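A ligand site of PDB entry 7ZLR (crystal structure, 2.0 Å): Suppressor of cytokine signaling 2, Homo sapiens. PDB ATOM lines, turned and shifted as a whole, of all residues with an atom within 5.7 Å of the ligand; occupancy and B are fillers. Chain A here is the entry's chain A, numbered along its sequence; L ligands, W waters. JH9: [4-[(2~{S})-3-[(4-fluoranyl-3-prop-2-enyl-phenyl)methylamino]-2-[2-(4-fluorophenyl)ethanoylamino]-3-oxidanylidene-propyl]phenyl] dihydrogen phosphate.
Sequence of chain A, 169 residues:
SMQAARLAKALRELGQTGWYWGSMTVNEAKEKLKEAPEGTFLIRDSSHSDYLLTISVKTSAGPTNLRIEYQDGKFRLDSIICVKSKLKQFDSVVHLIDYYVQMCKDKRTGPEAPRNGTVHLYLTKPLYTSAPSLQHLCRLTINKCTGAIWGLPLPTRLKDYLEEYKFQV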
ATOM      1  N   VAL A  26     -14.505 -20.981 -13.675  1.00  0.00           N
ATOM      2  CA  VAL A  26     -15.505 -21.576 -12.799  1.00  0.00           C
ATOM      3  C   VAL A  26     -16.372 -20.499 -12.149  1.00  0.00           C
ATOM      4  O   VAL A  26     -17.550 -20.720 -11.846  1.00  0.00           O
ATOM      5  CB  VAL A  26     -14.820 -22.487 -11.760  1.00  0.00           C
ATOM      6  CG1 VAL A  26     -13.967 -21.677 -10.821  1.00  0.00           C
ATOM      7  CG2 VAL A  26     -15.846 -23.285 -10.980  1.00  0.00           C
ATOM      8  N   ASN A  27     -15.814 -19.288 -11.950  1.00  0.00           N
ATOM      9  CA  ASN A  27     -16.550 -18.196 -11.310  1.00  0.00           C
ATOM     10  C   ASN A  27     -17.414 -17.421 -12.286  1.00  0.00           C
ATOM     11  O   ASN A  27     -18.453 -16.871 -11.895  1.00  0.00           O
ATOM     12  CB  ASN A  27     -15.586 -17.253 -10.612  1.00  0.00           C
ATOM     13  CG  ASN A  27     -14.963 -17.860  -9.380  1.00  0.00           C
ATOM     14  OD1 ASN A  27     -15.654 -18.078  -8.386  1.00  0.00           O
ATOM     15  ND2 ASN A  27     -13.665 -18.120  -9.435  1.00  0.00           N
ATOM     16  N   LYS A  30     -20.385 -19.569 -12.395  1.00  0.00           N
ATOM     17  CA  LYS A  30     -21.198 -19.354 -11.202  1.00  0.00           C
ATOM     18  C   LYS A  30     -22.059 -18.110 -11.347  1.00  0.00           C
ATOM     19  O   LYS A  30     -23.229 -18.099 -10.947  1.00  0.00           O
ATOM     20  CB  LYS A  30     -20.310 -19.246  -9.957  1.00  0.00           C
ATOM     21  CG  LYS A  30     -21.056 -18.923  -8.638  1.00  0.00           C
ATOM     22  CD  LYS A  30     -20.075 -18.662  -7.480  1.00  0.00           C
ATOM     23  CE  LYS A  30     -19.181 -17.456  -7.777  1.00  0.00           C
ATOM     24  NZ  LYS A  30     -18.394 -17.005  -6.581  1.00  0.00           N
ATOM     25  N   ARG A  44     -18.266 -26.260 -20.706  1.00  0.00           N
ATOM     26  CA  ARG A  44     -17.153 -25.365 -20.867  1.00  0.00           C
ATOM     27  C   ARG A  44     -15.861 -26.158 -20.728  1.00  0.00           C
ATOM     28  O   ARG A  44     -15.850 -27.312 -20.253  1.00  0.00           O
ATOM     29  CB  ARG A  44     -17.184 -24.224 -19.834  1.00  0.00           C
ATOM     30  CG  ARG A  44     -17.180 -24.730 -18.402  1.00  0.00           C
ATOM     31  CD  ARG A  44     -17.142 -23.605 -17.341  1.00  0.00           C
ATOM     32  NE  ARG A  44     -17.159 -24.154 -15.991  1.00  0.00           N
ATOM     33  CZ  ARG A  44     -16.101 -24.597 -15.321  1.00  0.00           C
ATOM     34  NH1 ARG A  44     -14.864 -24.510 -15.829  1.00  0.00           N
ATOM     35  NH2 ARG A  44     -16.268 -25.114 -14.111  1.00  0.00           N
ATOM     36  N   ASP A  45     -14.754 -25.540 -21.129  1.00  0.00           N
ATOM     37  CA  ASP A  45     -13.472 -26.169 -20.907  1.00  0.00           C
ATOM     38  C   ASP A  45     -13.217 -26.287 -19.413  1.00  0.00           C
ATOM     39  O   ASP A  45     -13.529 -25.369 -18.652  1.00  0.00           O
ATOM     40  CB  ASP A  45     -12.357 -25.358 -21.575  1.00  0.00           C
ATOM     41  CG  ASP A  45     -12.521 -25.270 -23.083  1.00  0.00           C
ATOM     42  OD1 ASP A  45     -13.398 -25.962 -23.662  1.00  0.00           O
ATOM     43  OD2 ASP A  45     -11.738 -24.507 -23.703  1.00  0.00           O
ATOM     44  N   SER A  46     -12.658 -27.414 -19.005  1.00  0.00           N
ATOM     45  CA  SER A  46     -12.173 -27.555 -17.628  1.00  0.00           C
ATOM     46  C   SER A  46     -10.895 -26.760 -17.421  1.00  0.00           C
ATOM     47  O   SER A  46     -10.033 -26.680 -18.316  1.00  0.00           O
ATOM     48  CB  SER A  46     -11.910 -29.023 -17.297  1.00  0.00           C
ATOM     49  OG  SER A  46     -11.284 -29.148 -16.012  1.00  0.00           O
ATOM     50  N   SER A  47     -10.756 -26.191 -16.222  1.00  0.00           N
ATOM     51  CA  SER A  47      -9.493 -25.620 -15.766  1.00  0.00           C
ATOM     52  C   SER A  47      -8.464 -26.680 -15.393  1.00  0.00           C
ATOM     53  O   SER A  47      -7.307 -26.338 -15.138  1.00  0.00           O
ATOM     54  CB  SER A  47      -9.717 -24.743 -14.527  1.00  0.00           C
ATOM     55  OG  SER A  47     -10.607 -23.668 -14.786  1.00  0.00           O
ATOM     56  N   HIS A  48      -8.860 -27.937 -15.280  1.00  0.00           N
ATOM     57  CA  HIS A  48      -7.973 -28.948 -14.727  1.00  0.00           C
ATOM     58  C   HIS A  48      -7.085 -29.527 -15.834  1.00  0.00           C
ATOM     59  O   HIS A  48      -7.545 -29.759 -16.954  1.00  0.00           O
ATOM     60  CB  HIS A  48      -8.791 -30.063 -14.062  1.00  0.00           C
ATOM     61  CG  HIS A  48      -7.971 -30.954 -13.174  1.00  0.00           C
ATOM     62  ND1 HIS A  48      -7.072 -31.863 -13.680  1.00  0.00           N
ATOM     63  CD2 HIS A  48      -7.907 -31.072 -11.828  1.00  0.00           C
ATOM     64  CE1 HIS A  48      -6.486 -32.502 -12.679  1.00  0.00           C
ATOM     65  NE2 HIS A  48      -6.980 -32.040 -11.539  1.00  0.00           N
ATOM     66  N   THR A  54     -16.006 -29.591 -18.690  1.00  0.00           N
ATOM     67  CA  THR A  54     -16.729 -29.644 -17.431  1.00  0.00           C
ATOM     68  C   THR A  54     -18.161 -29.195 -17.688  1.00  0.00           C
ATOM     69  O   THR A  54     -18.383 -28.223 -18.415  1.00  0.00           O
ATOM     70  CB  THR A  54     -16.094 -28.709 -16.410  1.00  0.00           C
ATOM     71  OG1 THR A  54     -14.787 -29.174 -16.067  1.00  0.00           O
ATOM     72  CG2 THR A  54     -16.955 -28.601 -15.165  1.00  0.00           C
ATOM     73  N   VAL A  57     -23.939 -26.626 -13.879  1.00  0.00           N
ATOM     74  CA  VAL A  57     -25.384 -26.823 -13.795  1.00  0.00           C
ATOM     75  C   VAL A  57     -25.927 -26.181 -12.522  1.00  0.00           C
ATOM     76  O   VAL A  57     -25.295 -26.257 -11.455  1.00  0.00           O
ATOM     77  CB  VAL A  57     -25.748 -28.332 -13.861  1.00  0.00           C
ATOM     78  CG1 VAL A  57     -24.914 -29.111 -12.862  1.00  0.00           C
ATOM     79  CG2 VAL A  57     -27.265 -28.588 -13.652  1.00  0.00           C
ATOM     80  N   THR A  59     -28.164 -26.219  -9.483  1.00  0.00           N
ATOM     81  CA  THR A  59     -28.987 -26.996  -8.558  1.00  0.00           C
ATOM     82  C   THR A  59     -29.785 -26.026  -7.695  1.00  0.00           C
ATOM     83  O   THR A  59     -29.630 -24.805  -7.781  1.00  0.00           O
ATOM     84  CB  THR A  59     -28.140 -27.935  -7.696  1.00  0.00           C
ATOM     85  OG1 THR A  59     -27.447 -27.194  -6.681  1.00  0.00           O
ATOM     86  CG2 THR A  59     -27.099 -28.661  -8.544  1.00  0.00           C
ATOM     87  N   PRO A  63     -25.144 -23.079  -8.337  1.00  0.00           N
ATOM     88  CA  PRO A  63     -24.478 -23.770  -9.444  1.00  0.00           C
ATOM     89  C   PRO A  63     -23.384 -24.688  -8.917  1.00  0.00           C
ATOM     90  O   PRO A  63     -22.767 -24.413  -7.897  1.00  0.00           O
ATOM     91  CB  PRO A  63     -23.892 -22.616 -10.277  1.00  0.00           C
ATOM     92  CG  PRO A  63     -24.437 -21.322  -9.646  1.00  0.00           C
ATOM     93  CD  PRO A  63     -24.738 -21.665  -8.241  1.00  0.00           C
ATOM     94  N   THR A  64     -23.189 -25.806  -9.619  1.00  0.00           N
ATOM     95  CA  THR A  64     -22.193 -26.798  -9.264  1.00  0.00           C
ATOM     96  C   THR A  64     -21.547 -27.283 -10.553  1.00  0.00           C
ATOM     97  O   THR A  64     -21.988 -26.952 -11.656  1.00  0.00           O
ATOM     98  CB  THR A  64     -22.815 -27.949  -8.451  1.00  0.00           C
ATOM     99  OG1 THR A  64     -21.777 -28.771  -7.900  1.00  0.00           O
ATOM    100  CG2 THR A  64     -23.725 -28.780  -9.295  1.00  0.00           C
ATOM    101  N   ASN A  65     -20.455 -28.045 -10.421  1.00  0.00           N
ATOM    102  CA  ASN A  65     -19.633 -28.381 -11.570  1.00  0.00           C
ATOM    103  C   ASN A  65     -19.305 -29.871 -11.590  1.00  0.00           C
ATOM    104  O   ASN A  65     -18.975 -30.450 -10.544  1.00  0.00           O
ATOM    105  CB  ASN A  65     -18.324 -27.589 -11.554  1.00  0.00           C
ATOM    106  CG  ASN A  65     -18.552 -26.084 -11.620  1.00  0.00           C
ATOM    107  OD1 ASN A  65     -18.534 -25.483 -12.698  1.00  0.00           O
ATOM    108  ND2 ASN A  65     -18.752 -25.461 -10.449  1.00  0.00           N
ATOM    109  N   LEU A  66     -19.337 -30.478 -12.773  1.00  0.00           N
ATOM    110  CA  LEU A  66     -19.071 -31.907 -12.941  1.00  0.00           C
ATOM    111  C   LEU A  66     -18.161 -32.092 -14.135  1.00  0.00           C
ATOM    112  O   LEU A  66     -18.517 -31.696 -15.245  1.00  0.00           O
ATOM    113  CB  LEU A  66     -20.383 -32.687 -13.140  1.00  0.00           C
ATOM    114  CG  LEU A  66     -20.396 -34.212 -13.167  1.00  0.00           C
ATOM    115  CD1 LEU A  66     -19.293 -34.843 -12.254  1.00  0.00           C
ATOM    116  CD2 LEU A  66     -21.792 -34.677 -12.761  1.00  0.00           C
ATOM    117  N   ARG A  67     -16.967 -32.643 -13.911  1.00  0.00           N
ATOM    118  CA  ARG A  67     -16.016 -32.802 -14.997  1.00  0.00           C
ATOM    119  C   ARG A  67     -16.393 -33.989 -15.879  1.00  0.00           C
ATOM    120  O   ARG A  67     -16.987 -34.959 -15.406  1.00  0.00           O
ATOM    121  CB  ARG A  67     -14.600 -32.987 -14.451  1.00  0.00           C
ATOM    122  CG  ARG A  67     -14.024 -31.695 -13.855  1.00  0.00           C
ATOM    123  CD  ARG A  67     -12.642 -31.909 -13.223  1.00  0.00           C
ATOM    124  NE  ARG A  67     -12.168 -30.678 -12.597  1.00  0.00           N
ATOM    125  CZ  ARG A  67     -11.680 -30.593 -11.369  1.00  0.00           C
ATOM    126  NH1 ARG A  67     -11.488 -31.678 -10.630  1.00  0.00           N
ATOM    127  NH2 ARG A  67     -11.380 -29.400 -10.871  1.00  0.00           N
ATOM    128  N   ILE A  81     -16.905 -39.655  -8.902  1.00  0.00           N
ATOM    129  CA  ILE A  81     -18.174 -39.504  -8.213  1.00  0.00           C
ATOM    130  C   ILE A  81     -18.927 -40.817  -8.016  1.00  0.00           C
ATOM    131  O   ILE A  81     -19.788 -40.911  -7.119  1.00  0.00           O
ATOM    132  CB  ILE A  81     -19.038 -38.486  -8.983  1.00  0.00           C
ATOM    133  CG1 ILE A  81     -19.652 -39.134 -10.222  1.00  0.00           C
ATOM    134  CG2 ILE A  81     -18.174 -37.265  -9.360  1.00  0.00           C
ATOM    135  N   VAL A 119     -25.825 -42.442  -9.951  1.00  0.00           N
ATOM    136  CA  VAL A 119     -25.524 -41.106 -10.438  1.00  0.00           C
ATOM    137  C   VAL A 119     -26.751 -40.200 -10.301  1.00  0.00           C
ATOM    138  O   VAL A 119     -27.889 -40.627 -10.547  1.00  0.00           O
ATOM    139  CB  VAL A 119     -25.037 -41.191 -11.894  1.00  0.00           C
ATOM    140  CG1 VAL A 119     -25.970 -42.103 -12.707  1.00  0.00           C
ATOM    141  CG2 VAL A 119     -24.941 -39.803 -12.520  1.00  0.00           C
ATOM    142  N   HIS A 120     -26.527 -38.946  -9.899  1.00  0.00           N
ATOM    143  CA  HIS A 120     -27.580 -37.941  -9.742  1.00  0.00           C
ATOM    144  C   HIS A 120     -27.255 -36.680 -10.550  1.00  0.00           C
ATOM    145  O   HIS A 120     -26.539 -35.797 -10.062  1.00  0.00           O
ATOM    146  CB  HIS A 120     -27.801 -37.557  -8.280  1.00  0.00           C
ATOM    147  CG  HIS A 120     -28.780 -36.440  -8.110  1.00  0.00           C
ATOM    148  ND1 HIS A 120     -30.065 -36.483  -8.619  1.00  0.00           N
ATOM    149  CD2 HIS A 120     -28.652 -35.226  -7.506  1.00  0.00           C
ATOM    150  CE1 HIS A 120     -30.697 -35.355  -8.327  1.00  0.00           C
ATOM    151  NE2 HIS A 120     -29.862 -34.583  -7.658  1.00  0.00           N
ATOM    152  N   LEU A 121     -27.806 -36.574 -11.748  1.00  0.00           N
ATOM    153  CA  LEU A 121     -27.537 -35.447 -12.623  1.00  0.00           C
ATOM    154  C   LEU A 121     -28.858 -34.935 -13.156  1.00  0.00           C
ATOM    155  O   LEU A 121     -29.464 -35.560 -14.040  1.00  0.00           O
ATOM    156  CB  LEU A 121     -26.603 -35.844 -13.758  1.00  0.00           C
ATOM    157  CG  LEU A 121     -26.055 -34.681 -14.576  1.00  0.00           C
ATOM    158  CD1 LEU A 121     -25.534 -33.580 -13.668  1.00  0.00           C
ATOM    159  CD2 LEU A 121     -24.982 -35.169 -15.544  1.00  0.00           C
ATOM    160  N   TYR A 122     -29.326 -33.797 -12.648  1.00  0.00           N
ATOM    161  CA  TYR A 122     -30.612 -33.248 -13.051  1.00  0.00           C
ATOM    162  C   TYR A 122     -30.353 -32.146 -14.075  1.00  0.00           C
ATOM    163  O   TYR A 122     -29.854 -31.067 -13.721  1.00  0.00           O
ATOM    164  CB  TYR A 122     -31.391 -32.743 -11.841  1.00  0.00           C
ATOM    165  CG  TYR A 122     -32.772 -32.223 -12.195  1.00  0.00           C
ATOM    166  CD1 TYR A 122     -33.762 -33.085 -12.656  1.00  0.00           C
ATOM    167  CD2 TYR A 122     -33.072 -30.869 -12.087  1.00  0.00           C
ATOM    168  CE1 TYR A 122     -35.021 -32.602 -12.983  1.00  0.00           C
ATOM    169  CE2 TYR A 122     -34.338 -30.387 -12.419  1.00  0.00           C
ATOM    170  CZ  TYR A 122     -35.305 -31.259 -12.860  1.00  0.00           C
ATOM    171  OH  TYR A 122     -36.546 -30.793 -13.206  1.00  0.00           O
HETATM  172  C10 JH9 L   1     -19.136 -24.502  -7.168  1.00  0.00           C
HETATM  173  C13 JH9 L   1     -18.063 -30.892  -7.198  1.00  0.00           C
HETATM  174  C15 JH9 L   1     -19.716 -32.753  -7.224  1.00  0.00           C
HETATM  175  C17 JH9 L   1     -20.913 -34.680  -8.247  1.00  0.00           C
HETATM  176  C21 JH9 L   1     -22.891 -33.033  -9.345  1.00  0.00           C
HETATM  177  C22 JH9 L   1     -24.017 -32.185  -9.985  1.00  0.00           C
HETATM  178  C24 JH9 L   1     -26.535 -32.064  -9.905  1.00  0.00           C
HETATM  179  C28 JH9 L   1     -15.446 -29.107  -9.349  1.00  0.00           C
HETATM  180  C02 JH9 L   1     -18.104 -27.548  -7.008  1.00  0.00           C
HETATM  181  C03 JH9 L   1     -18.099 -26.453  -5.948  1.00  0.00           C
HETATM  182  C04 JH9 L   1     -18.006 -25.076  -6.602  1.00  0.00           C
HETATM  183  C05 JH9 L   1     -16.783 -24.405  -6.616  1.00  0.00           C
HETATM  184  C06 JH9 L   1     -16.698 -23.147  -7.204  1.00  0.00           C
HETATM  185  C07 JH9 L   1     -17.823 -22.581  -7.773  1.00  0.00           C
HETATM  186  C09 JH9 L   1     -19.039 -23.250  -7.754  1.00  0.00           C
HETATM  187  C12 JH9 L   1     -17.308 -29.725  -7.839  1.00  0.00           C
HETATM  188  C16 JH9 L   1     -20.869 -33.312  -8.046  1.00  0.00           C
HETATM  189  C18 JH9 L   1     -21.942 -35.244  -8.982  1.00  0.00           C
HETATM  190  C19 JH9 L   1     -22.923 -34.419  -9.525  1.00  0.00           C
HETATM  191  C23 JH9 L   1     -25.378 -32.177  -9.246  1.00  0.00           C
HETATM  192  C25 JH9 L   1     -21.846 -32.481  -8.596  1.00  0.00           C
HETATM  193  C27 JH9 L   1     -15.879 -30.059  -8.222  1.00  0.00           C
HETATM  194  C29 JH9 L   1     -15.326 -29.633 -10.616  1.00  0.00           C
HETATM  195  C30 JH9 L   1     -14.942 -28.827 -11.667  1.00  0.00           C
HETATM  196  C31 JH9 L   1     -14.693 -27.495 -11.447  1.00  0.00           C
HETATM  197  C37 JH9 L   1     -14.817 -26.948 -10.178  1.00  0.00           C
HETATM  198  C38 JH9 L   1     -15.210 -27.766  -9.113  1.00  0.00           C
HETATM  199  F08 JH9 L   1     -17.755 -21.336  -8.353  1.00  0.00           F
HETATM  200  F20 JH9 L   1     -23.916 -34.989 -10.257  1.00  0.00           F
HETATM  201  N11 JH9 L   1     -17.267 -28.709  -6.830  1.00  0.00           N
HETATM  202  N14 JH9 L   1     -19.055 -31.669  -7.925  1.00  0.00           N
HETATM  203  O01 JH9 L   1     -18.773 -27.471  -7.977  1.00  0.00           O
HETATM  204  O26 JH9 L   1     -17.858 -31.157  -6.062  1.00  0.00           O
HETATM  205  O32 JH9 L   1     -14.340 -26.711 -12.537  1.00  0.00           O
HETATM  206  O34 JH9 L   1     -13.064 -28.399 -14.100  1.00  0.00           O
HETATM  207  O35 JH9 L   1     -11.787 -27.084 -12.497  1.00  0.00           O
HETATM  208  O36 JH9 L   1     -12.880 -25.930 -14.446  1.00  0.00           O
HETATM  209  P33 JH9 L   1     -12.982 -27.048 -13.444  1.00  0.00           P
HETATM  210  O   HOH W   1     -11.560 -25.818 -10.357  1.00  0.00           O
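The side-chain hydroxyl (OG) of Ser 46 sits at hydrogen-bond distance from the backbone NH (N) of His 48. The backbone NH (N) of Thr 54 lies within hydrogen-bond range of the backbone carbonyl oxygen (O) of Arg 44 (2.8 Å). The side-chain amide oxygen (OD1) of Asn 65 sits at hydrogen-bond distance from the guanidinium group (NH2) of Arg 44, at 2.7 Å. N of Thr 64 lies within hydrogen-bond range of O of Val 57. OD1 of Asn 27 sits at hydrogen-bond distance from NZ of Lys 30.
An oxygen (O34) of the ligand sits at hydrogen-bond distance from the side-chain hydroxyl (OG) of Ser 46 (2.7 Å). OG1 of Thr 54 sits at hydrogen-bond distance from O34 of the ligand. O36 of the ligand lies within hydrogen-bond range of N of Ser 47. OG of Ser 47 lies within hydrogen-bond range of O36 of the ligand. O36 of the ligand is in salt-bridge range of NH1 of Arg 44 (2.8 Å). An oxygen (O35) of the ligand lies within salt-bridge range of the guanidinium group (NH2) of Arg 67. The backbone NH of Asn 65 sits at hydrogen-bond distance from an oxygen (O01) of the ligand. N14 of the ligand sits at hydrogen-bond distance from O of Asn 65 (2.9 Å). ND2 of Asn 65 sits at hydrogen-bond distance from O01 of the ligand. An oxygen (O01) of the ligand lies within hydrogen-bond range of the side-chain hydroxyl (OG1) of Thr 64 (3.3 Å).
The backbone carbonyl oxygen (O) of His 120 lies close to a fluorine (F20) of the ligand, at 2.8 Å. Residues that only touch the ligand: Val 26 (3.6 Å), Asn 27 (3.9 Å), Lys 30 (3.6 Å), Thr 59 (3.7 Å), Pro 63 (3.7 Å), Leu 66 (3.3 Å) and Ile 81 (3.9 Å). 15 residues have an atom within 4 Å of the ligand: Val 26, Asn 27, Lys 30, Arg 44, Ser 46, Ser 47, Thr 54, Thr 59, Pro 63, Thr 64, Asn 65, Leu 66, Arg 67, Ile 81 and His 120.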
